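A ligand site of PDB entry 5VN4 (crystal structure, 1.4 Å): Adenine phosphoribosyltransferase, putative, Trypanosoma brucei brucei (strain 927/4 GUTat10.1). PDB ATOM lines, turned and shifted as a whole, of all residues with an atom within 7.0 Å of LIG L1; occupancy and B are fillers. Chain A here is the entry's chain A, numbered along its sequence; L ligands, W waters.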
ATOM      1  N   TYR A  35     -16.428   3.229 -11.749  1.00  0.00           N
ATOM      2  CA  TYR A  35     -15.917   4.600 -11.703  1.00  0.00           C
ATOM      3  C   TYR A  35     -16.143   5.238 -13.072  1.00  0.00           C
ATOM      4  O   TYR A  35     -15.764   4.667 -14.107  1.00  0.00           O
ATOM      5  CB  TYR A  35     -14.435   4.622 -11.321  1.00  0.00           C
ATOM      6  CG  TYR A  35     -14.052   5.516 -10.139  1.00  0.00           C
ATOM      7  CD1 TYR A  35     -14.739   6.701  -9.851  1.00  0.00           C
ATOM      8  CD2 TYR A  35     -12.997   5.177  -9.315  1.00  0.00           C
ATOM      9  CE1 TYR A  35     -14.361   7.512  -8.777  1.00  0.00           C
ATOM     10  CE2 TYR A  35     -12.617   5.966  -8.244  1.00  0.00           C
ATOM     11  CZ  TYR A  35     -13.303   7.126  -7.973  1.00  0.00           C
ATOM     12  OH  TYR A  35     -12.892   7.885  -6.901  1.00  0.00           O
ATOM     13  N   HIS A  45     -16.036  21.046 -11.832  1.00  0.00           N
ATOM     14  CA  HIS A  45     -14.695  21.608 -11.921  1.00  0.00           C
ATOM     15  C   HIS A  45     -14.036  21.185 -13.226  1.00  0.00           C
ATOM     16  O   HIS A  45     -13.996  19.993 -13.515  1.00  0.00           O
ATOM     17  CB  HIS A  45     -13.836  21.127 -10.758  1.00  0.00           C
ATOM     18  CG  HIS A  45     -14.390  21.494  -9.434  1.00  0.00           C
ATOM     19  ND1 HIS A  45     -14.426  22.800  -8.971  1.00  0.00           N
ATOM     20  CD2 HIS A  45     -14.964  20.743  -8.469  1.00  0.00           C
ATOM     21  CE1 HIS A  45     -14.988  22.819  -7.778  1.00  0.00           C
ATOM     22  NE2 HIS A  45     -15.319  21.587  -7.443  1.00  0.00           N
ATOM     23  N   VAL A  47     -11.463  20.111 -14.745  1.00  0.00           N
ATOM     24  CA  VAL A  47     -10.301  19.251 -14.953  1.00  0.00           C
ATOM     25  C   VAL A  47     -10.669  18.386 -16.142  1.00  0.00           C
ATOM     26  O   VAL A  47     -11.858  18.294 -16.482  1.00  0.00           O
ATOM     27  CB  VAL A  47     -10.023  18.411 -13.692  1.00  0.00           C
ATOM     28  CG1 VAL A  47      -9.634  19.307 -12.519  1.00  0.00           C
ATOM     29  CG2 VAL A  47     -11.239  17.550 -13.332  1.00  0.00           C
ATOM     30  N   PRO A  48      -9.716  17.757 -16.838  1.00  0.00           N
ATOM     31  CA  PRO A  48     -10.108  16.940 -17.996  1.00  0.00           C
ATOM     32  C   PRO A  48     -11.069  15.811 -17.662  1.00  0.00           C
ATOM     33  O   PRO A  48     -12.037  15.572 -18.400  1.00  0.00           O
ATOM     34  CB  PRO A  48      -8.761  16.401 -18.509  1.00  0.00           C
ATOM     35  CG  PRO A  48      -7.748  17.382 -18.027  1.00  0.00           C
ATOM     36  CD  PRO A  48      -8.258  17.885 -16.703  1.00  0.00           C
ATOM     37  N   ARG A  49     -10.834  15.124 -16.553  1.00  0.00           N
ATOM     38  CA  ARG A  49     -11.622  13.928 -16.206  1.00  0.00           C
ATOM     39  C   ARG A  49     -11.938  13.996 -14.719  1.00  0.00           C
ATOM     40  O   ARG A  49     -11.071  13.754 -13.875  1.00  0.00           O
ATOM     41  CB  ARG A  49     -10.878  12.648 -16.600  1.00  0.00           C
ATOM     42  CG  ARG A  49     -10.536  12.627 -18.084  1.00  0.00           C
ATOM     43  CD  ARG A  49     -10.164  11.255 -18.670  1.00  0.00           C
ATOM     44  NE  ARG A  49     -10.074  11.379 -20.128  1.00  0.00           N
ATOM     45  CZ  ARG A  49     -10.087  10.375 -20.994  1.00  0.00           C
ATOM     46  NH1 ARG A  49     -10.164   9.114 -20.584  1.00  0.00           N
ATOM     47  NH2 ARG A  49     -10.015  10.632 -22.301  1.00  0.00           N
ATOM     48  N   PHE A  50     -13.182  14.329 -14.391  1.00  0.00           N
ATOM     49  CA  PHE A  50     -13.628  14.452 -13.014  1.00  0.00           C
ATOM     50  C   PHE A  50     -14.282  13.157 -12.564  1.00  0.00           C
ATOM     51  O   PHE A  50     -15.291  12.736 -13.126  1.00  0.00           O
ATOM     52  CB  PHE A  50     -14.608  15.614 -12.874  1.00  0.00           C
ATOM     53  CG  PHE A  50     -15.077  15.833 -11.454  1.00  0.00           C
ATOM     54  CD1 PHE A  50     -14.344  16.633 -10.587  1.00  0.00           C
ATOM     55  CD2 PHE A  50     -16.230  15.232 -10.982  1.00  0.00           C
ATOM     56  CE1 PHE A  50     -14.768  16.829  -9.276  1.00  0.00           C
ATOM     57  CE2 PHE A  50     -16.653  15.438  -9.681  1.00  0.00           C
ATOM     58  CZ  PHE A  50     -15.918  16.227  -8.826  1.00  0.00           C
ATOM     59  N   ALA A  51     -13.722  12.552 -11.516  1.00  0.00           N
ATOM     60  CA  ALA A  51     -14.163  11.246 -11.038  1.00  0.00           C
ATOM     61  C   ALA A  51     -15.192  11.442  -9.930  1.00  0.00           C
ATOM     62  O   ALA A  51     -14.852  11.699  -8.773  1.00  0.00           O
ATOM     63  CB  ALA A  51     -12.972  10.437 -10.558  1.00  0.00           C
ATOM     64  N   GLU A  52     -16.475  11.289 -10.284  1.00  0.00           N
ATOM     65  CA  GLU A  52     -17.570  11.544  -9.351  1.00  0.00           C
ATOM     66  C   GLU A  52     -17.659  10.431  -8.308  1.00  0.00           C
ATOM     67  O   GLU A  52     -17.860   9.257  -8.628  1.00  0.00           O
ATOM     68  CB  GLU A  52     -18.877  11.644 -10.139  1.00  0.00           C
ATOM     69  CG  GLU A  52     -20.157  11.632  -9.303  1.00  0.00           C
ATOM     70  CD  GLU A  52     -20.229  12.756  -8.296  1.00  0.00           C
ATOM     71  OE1 GLU A  52     -19.948  13.923  -8.678  1.00  0.00           O
ATOM     72  OE2 GLU A  52     -20.569  12.481  -7.120  1.00  0.00           O
ATOM     73  N   VAL A  53     -17.547  10.810  -7.029  1.00  0.00           N
ATOM     74  CA  VAL A  53     -17.554   9.798  -5.970  1.00  0.00           C
ATOM     75  C   VAL A  53     -18.920   9.143  -5.796  1.00  0.00           C
ATOM     76  O   VAL A  53     -19.005   8.017  -5.264  1.00  0.00           O
ATOM     77  CB  VAL A  53     -17.075  10.432  -4.637  1.00  0.00           C
ATOM     78  CG1 VAL A  53     -18.186  11.253  -4.015  1.00  0.00           C
ATOM     79  CG2 VAL A  53     -16.555   9.365  -3.682  1.00  0.00           C
ATOM     80  N   ARG A  90     -15.841  14.645   0.936  1.00  0.00           N
ATOM     81  CA  ARG A  90     -15.875  13.301   0.358  1.00  0.00           C
ATOM     82  C   ARG A  90     -15.121  12.286   1.211  1.00  0.00           C
ATOM     83  O   ARG A  90     -15.492  11.108   1.215  1.00  0.00           O
ATOM     84  CB  ARG A  90     -15.422  13.342  -1.100  1.00  0.00           C
ATOM     85  CG  ARG A  90     -16.453  14.061  -1.981  1.00  0.00           C
ATOM     86  CD  ARG A  90     -16.082  13.990  -3.446  1.00  0.00           C
ATOM     87  NE  ARG A  90     -15.506  15.229  -3.934  1.00  0.00           N
ATOM     88  CZ  ARG A  90     -14.605  15.299  -4.909  1.00  0.00           C
ATOM     89  NH1 ARG A  90     -14.143  14.192  -5.474  1.00  0.00           N
ATOM     90  NH2 ARG A  90     -14.177  16.481  -5.326  1.00  0.00           N
ATOM     91  N   LYS A 127      -5.882  22.862  -4.416  1.00  0.00           N
ATOM     92  CA  LYS A 127      -6.331  21.589  -4.971  1.00  0.00           C
ATOM     93  C   LYS A 127      -6.061  21.609  -6.468  1.00  0.00           C
ATOM     94  O   LYS A 127      -5.769  22.657  -7.040  1.00  0.00           O
ATOM     95  CB  LYS A 127      -7.830  21.349  -4.718  1.00  0.00           C
ATOM     96  CG  LYS A 127      -8.278  21.335  -3.251  1.00  0.00           C
ATOM     97  CD  LYS A 127      -9.803  21.229  -3.193  1.00  0.00           C
ATOM     98  CE  LYS A 127     -10.329  20.975  -1.782  1.00  0.00           C
ATOM     99  NZ  LYS A 127     -10.060  19.596  -1.304  1.00  0.00           N
ATOM    100  N   GLU A 128      -6.232  20.445  -7.120  1.00  0.00           N
ATOM    101  CA  GLU A 128      -6.076  20.389  -8.576  1.00  0.00           C
ATOM    102  C   GLU A 128      -6.849  21.515  -9.258  1.00  0.00           C
ATOM    103  O   GLU A 128      -6.370  22.113 -10.234  1.00  0.00           O
ATOM    104  CB  GLU A 128      -6.531  19.024  -9.107  1.00  0.00           C
ATOM    105  CG  GLU A 128      -6.258  18.841 -10.612  1.00  0.00           C
ATOM    106  CD  GLU A 128      -6.858  17.582 -11.238  1.00  0.00           C
ATOM    107  OE1 GLU A 128      -7.571  16.816 -10.551  1.00  0.00           O
ATOM    108  OE2 GLU A 128      -6.624  17.346 -12.439  1.00  0.00           O
ATOM    109  N   TYR A 129      -8.037  21.832  -8.739  1.00  0.00           N
ATOM    110  CA  TYR A 129      -8.907  22.825  -9.356  1.00  0.00           C
ATOM    111  C   TYR A 129      -9.127  24.069  -8.505  1.00  0.00           C
ATOM    112  O   TYR A 129     -10.048  24.838  -8.780  1.00  0.00           O
ATOM    113  CB  TYR A 129     -10.244  22.196  -9.755  1.00  0.00           C
ATOM    114  CG  TYR A 129     -10.945  21.392  -8.679  1.00  0.00           C
ATOM    115  CD1 TYR A 129     -11.498  22.006  -7.566  1.00  0.00           C
ATOM    116  CD2 TYR A 129     -11.096  20.016  -8.817  1.00  0.00           C
ATOM    117  CE1 TYR A 129     -12.181  21.267  -6.597  1.00  0.00           C
ATOM    118  CE2 TYR A 129     -11.776  19.276  -7.871  1.00  0.00           C
ATOM    119  CZ  TYR A 129     -12.303  19.903  -6.763  1.00  0.00           C
ATOM    120  OH  TYR A 129     -12.987  19.147  -5.835  1.00  0.00           O
ATOM    121  N   ASP A 155     -11.126  10.841  -0.687  1.00  0.00           N
ATOM    122  CA  ASP A 155     -11.437  10.031  -1.863  1.00  0.00           C
ATOM    123  C   ASP A 155     -10.327  10.098  -2.920  1.00  0.00           C
ATOM    124  O   ASP A 155      -9.758   9.069  -3.288  1.00  0.00           O
ATOM    125  CB  ASP A 155     -12.847  10.318  -2.433  1.00  0.00           C
ATOM    126  CG  ASP A 155     -12.977  11.680  -3.090  1.00  0.00           C
ATOM    127  OD1 ASP A 155     -12.343  12.654  -2.626  1.00  0.00           O
ATOM    128  OD2 ASP A 155     -13.774  11.773  -4.068  1.00  0.00           O
ATOM    129  N   VAL A 156      -9.989  11.296  -3.380  1.00  0.00           N
ATOM    130  CA  VAL A 156      -9.025  11.499  -4.466  1.00  0.00           C
ATOM    131  C   VAL A 156      -7.798  12.181  -3.897  1.00  0.00           C
ATOM    132  O   VAL A 156      -7.901  13.128  -3.108  1.00  0.00           O
ATOM    133  CB  VAL A 156      -9.649  12.368  -5.583  1.00  0.00           C
ATOM    134  CG1 VAL A 156      -8.604  12.645  -6.685  1.00  0.00           C
ATOM    135  CG2 VAL A 156     -10.882  11.692  -6.166  1.00  0.00           C
ATOM    136  N   ILE A 157      -6.624  11.721  -4.324  1.00  0.00           N
ATOM    137  CA  ILE A 157      -5.364  12.443  -4.150  1.00  0.00           C
ATOM    138  C   ILE A 157      -4.889  12.842  -5.539  1.00  0.00           C
ATOM    139  O   ILE A 157      -4.626  11.984  -6.385  1.00  0.00           O
ATOM    140  CB  ILE A 157      -4.315  11.614  -3.403  1.00  0.00           C
ATOM    141  CG1 ILE A 157      -4.833  11.227  -2.005  1.00  0.00           C
ATOM    142  CG2 ILE A 157      -3.012  12.418  -3.293  1.00  0.00           C
ATOM    143  CD1 ILE A 157      -3.970  10.267  -1.262  1.00  0.00           C
ATOM    144  N   ALA A 158      -4.836  14.156  -5.782  1.00  0.00           N
ATOM    145  CA  ALA A 158      -4.466  14.694  -7.075  1.00  0.00           C
ATOM    146  C   ALA A 158      -3.149  15.434  -6.896  1.00  0.00           C
ATOM    147  O   ALA A 158      -2.086  14.798  -6.887  1.00  0.00           O
ATOM    148  CB  ALA A 158      -5.622  15.531  -7.659  1.00  0.00           C
ATOM    149  N   THR A 159      -3.165  16.762  -6.708  1.00  0.00           N
ATOM    150  CA  THR A 159      -1.910  17.480  -6.453  1.00  0.00           C
ATOM    151  C   THR A 159      -1.345  17.199  -5.073  1.00  0.00           C
ATOM    152  O   THR A 159      -0.164  17.490  -4.841  1.00  0.00           O
ATOM    153  CB  THR A 159      -2.125  18.987  -6.562  1.00  0.00           C
ATOM    154  OG1 THR A 159      -2.963  19.448  -5.488  1.00  0.00           O
ATOM    155  CG2 THR A 159      -2.716  19.371  -7.899  1.00  0.00           C
ATOM    156  N   THR A 162      -4.554  19.078  -0.664  1.00  0.00           N
ATOM    157  CA  THR A 162      -5.445  18.804   0.455  1.00  0.00           C
ATOM    158  C   THR A 162      -4.740  17.957   1.507  1.00  0.00           C
ATOM    159  O   THR A 162      -4.805  18.269   2.703  1.00  0.00           O
ATOM    160  CB  THR A 162      -6.723  18.125  -0.050  1.00  0.00           C
ATOM    161  OG1 THR A 162      -7.347  18.964  -1.039  1.00  0.00           O
ATOM    162  CG2 THR A 162      -7.710  17.885   1.110  1.00  0.00           C
ATOM    163  N   LEU A 184      -8.605   6.946  -5.134  1.00  0.00           N
ATOM    164  CA  LEU A 184      -8.134   7.293  -6.476  1.00  0.00           C
ATOM    165  C   LEU A 184      -6.930   8.207  -6.344  1.00  0.00           C
ATOM    166  O   LEU A 184      -7.023   9.303  -5.771  1.00  0.00           O
ATOM    167  CB  LEU A 184      -9.242   7.995  -7.265  1.00  0.00           C
ATOM    168  CG  LEU A 184      -8.831   8.510  -8.645  1.00  0.00           C
ATOM    169  CD1 LEU A 184      -8.394   7.371  -9.563  1.00  0.00           C
ATOM    170  CD2 LEU A 184      -9.978   9.268  -9.266  1.00  0.00           C
ATOM    171  N   LEU A 186      -4.054  10.177  -8.652  1.00  0.00           N
ATOM    172  CA  LEU A 186      -3.672  10.567 -10.006  1.00  0.00           C
ATOM    173  C   LEU A 186      -2.156  10.678  -9.984  1.00  0.00           C
ATOM    174  O   LEU A 186      -1.589  11.743  -9.702  1.00  0.00           O
ATOM    175  CB  LEU A 186      -4.358  11.863 -10.411  1.00  0.00           C
ATOM    176  CG  LEU A 186      -5.892  11.815 -10.297  1.00  0.00           C
ATOM    177  CD1 LEU A 186      -6.511  13.149 -10.674  1.00  0.00           C
ATOM    178  CD2 LEU A 186      -6.484  10.703 -11.154  1.00  0.00           C
ATOM    179  N   LEU A 189       0.339  13.415 -11.227  1.00  0.00           N
ATOM    180  CA  LEU A 189       0.442  14.675 -10.512  1.00  0.00           C
ATOM    181  C   LEU A 189       1.393  14.618  -9.328  1.00  0.00           C
ATOM    182  O   LEU A 189       1.635  15.646  -8.696  1.00  0.00           O
ATOM    183  CB  LEU A 189      -0.954  15.159 -10.055  1.00  0.00           C
ATOM    184  CG  LEU A 189      -1.946  15.450 -11.190  1.00  0.00           C
ATOM    185  CD1 LEU A 189      -3.311  15.805 -10.620  1.00  0.00           C
ATOM    186  CD2 LEU A 189      -1.443  16.569 -12.082  1.00  0.00           C
ATOM    187  N   LEU A 217      -9.714   5.804 -15.380  1.00  0.00           N
ATOM    188  CA  LEU A 217     -10.420   6.858 -16.108  1.00  0.00           C
ATOM    189  C   LEU A 217     -10.224   6.714 -17.617  1.00  0.00           C
ATOM    190  O   LEU A 217      -9.748   7.616 -18.308  1.00  0.00           O
ATOM    191  CB  LEU A 217      -9.991   8.219 -15.595  1.00  0.00           C
ATOM    192  CG  LEU A 217     -10.113   8.424 -14.083  1.00  0.00           C
ATOM    193  CD1 LEU A 217      -9.681   9.830 -13.680  1.00  0.00           C
ATOM    194  CD2 LEU A 217     -11.536   8.161 -13.604  1.00  0.00           C
HETATM  195  N1  LIG L   1     -10.525  16.197  -6.727  1.00  0.00           N
HETATM  196  C1  LIG L   1      -9.375  16.698  -7.259  1.00  0.00           C
HETATM  197  N2  LIG L   1      -9.166  16.331  -8.506  1.00  0.00           N
HETATM  198  C2  LIG L   1     -10.246  15.529  -8.810  1.00  0.00           C
HETATM  199  C3  LIG L   1     -10.627  14.830  -9.984  1.00  0.00           C
HETATM  200  N3  LIG L   1      -9.893  14.828 -11.121  1.00  0.00           N
HETATM  201  N4  LIG L   1     -11.776  14.135  -9.944  1.00  0.00           N
HETATM  202  C4  LIG L   1     -12.488  14.136  -8.817  1.00  0.00           C
HETATM  203  N5  LIG L   1     -12.255  14.756  -7.662  1.00  0.00           N
HETATM  204  C5  LIG L   1     -11.098  15.441  -7.722  1.00  0.00           C
HETATM  205  C1  LG2 L   2     -11.285  17.248  -3.888  1.00  0.00           C
HETATM  206  O1  LG2 L   2      -9.924  17.699  -3.952  1.00  0.00           O
HETATM  207  C2  LG2 L   2     -11.168  15.825  -3.398  1.00  0.00           C
HETATM  208  O2  LG2 L   2     -12.374  15.363  -2.772  1.00  0.00           O
HETATM  209  C3  LG2 L   2      -9.991  15.892  -2.452  1.00  0.00           C
HETATM  210  O3  LG2 L   2     -10.373  16.456  -1.177  1.00  0.00           O
HETATM  211  C4  LG2 L   2      -9.068  16.879  -3.147  1.00  0.00           C
HETATM  212  C5  LG2 L   2      -7.997  16.201  -4.007  1.00  0.00           C
HETATM  213  O4  LG2 L   2      -7.282  17.174  -4.768  1.00  0.00           O
HETATM  214  P1  LG2 L   2      -5.784  17.627  -4.364  1.00  0.00           P
HETATM  215  O5  LG2 L   2      -5.869  18.543  -3.144  1.00  0.00           O
HETATM  216  O6  LG2 L   2      -4.998  16.378  -4.102  1.00  0.00           O
HETATM  217  O7  LG2 L   2      -5.321  18.357  -5.601  1.00  0.00           O
HETATM  218  O8  LG2 L   2     -12.006  18.051  -2.940  1.00  0.00           O
HETATM  219  O   HOH W   1      -8.306  15.430 -14.155  1.00  0.00           O
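NH2 of Arg 90 lies within hydrogen-bond range of OH of Tyr 129 (3.0 Å).
NH1 of Arg 90 is in salt-bridge range of OD2 of Asp 155, 2.8 Å away.
O of Leu 217 is in hydrogen-bond range of NH1 of Arg 49 (2.8 Å).
N of Leu 186 lies within hydrogen-bond range of O of Ile 157, at 3.0 Å.
Water W1 lies within hydrogen-bond range of OE2 of Glu 128, O of Arg 49 and N3 of LIG L1.
CG2 of Val 47 touches N3 of LIG L1, at 3.8 Å.
CE1 of Phe 50 touches C4 of LIG L1, 3.6 Å away.
CE2 of Tyr 129 touches N1 of LIG L1, 3.5 Å away.
CG2 of Val 156 touches N5 of LIG L1, at 3.7 Å.
CB of Ala 158 touches N2 of LIG L1, at 3.7 Å.
Leu 186 touches LIG L1.
Hydrophobic or aromatic side chains that line LIG L1: Val 47, Phe 50, Ala 51, Tyr 129, Val 156, Ala 158 and Leu 186.
The side-chain carboxylate of Glu 128 sits at hydrogen-bond distance from a nitrogen (N2) of LIG L1.
A nitrogen (N5) of LIG L1 sits at hydrogen-bond distance from the guanidinium group (NH1) of Arg 90.
A nitrogen (N4) of LIG L1 lies within hydrogen-bond range of the backbone NH of Ala 51 (3.0 Å).
The backbone carbonyl oxygen (O) of Arg 49 is in hydrogen-bond range of a nitrogen (N3) of LIG L1 (3.2 Å).
The backbone NH of Glu 128 sits at hydrogen-bond distance from an oxygen (O7) of LG2 L2, at 2.7 Å.
NH2 of Arg 90 lies close to O2 of LG2 L2, 3.3 Å away.
OH of Tyr 129 sits close to O8 of LG2 L2, at 3.2 Å.
An oxygen (O6) of LG2 L2 lies within hydrogen-bond range of the backbone NH of Ala 158, at 2.8 Å.
OD1 of Asp 155 sits at hydrogen-bond distance from O2 of LG2 L2 (2.7 Å).
NZ of Lys 127 lies within hydrogen-bond range of O8 of LG2 L2, 3.0 Å away.
The backbone NH (N) of Thr 159 is in hydrogen-bond range of an oxygen (O7) of LG2 L2 (2.9 Å).
OG1 of Thr 159 sits at hydrogen-bond distance from O7 of LG2 L2 (2.6 Å).
An oxygen (O5) of LG2 L2 lies within hydrogen-bond range of the backbone NH of Thr 162.
OG1 of Thr 162 is in hydrogen-bond range of O5 of LG2 L2, 2.6 Å away.
A nitrogen (N1) of LIG L1 lies close to an oxygen (O1) of LG2 L2, at 3.2 Å.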
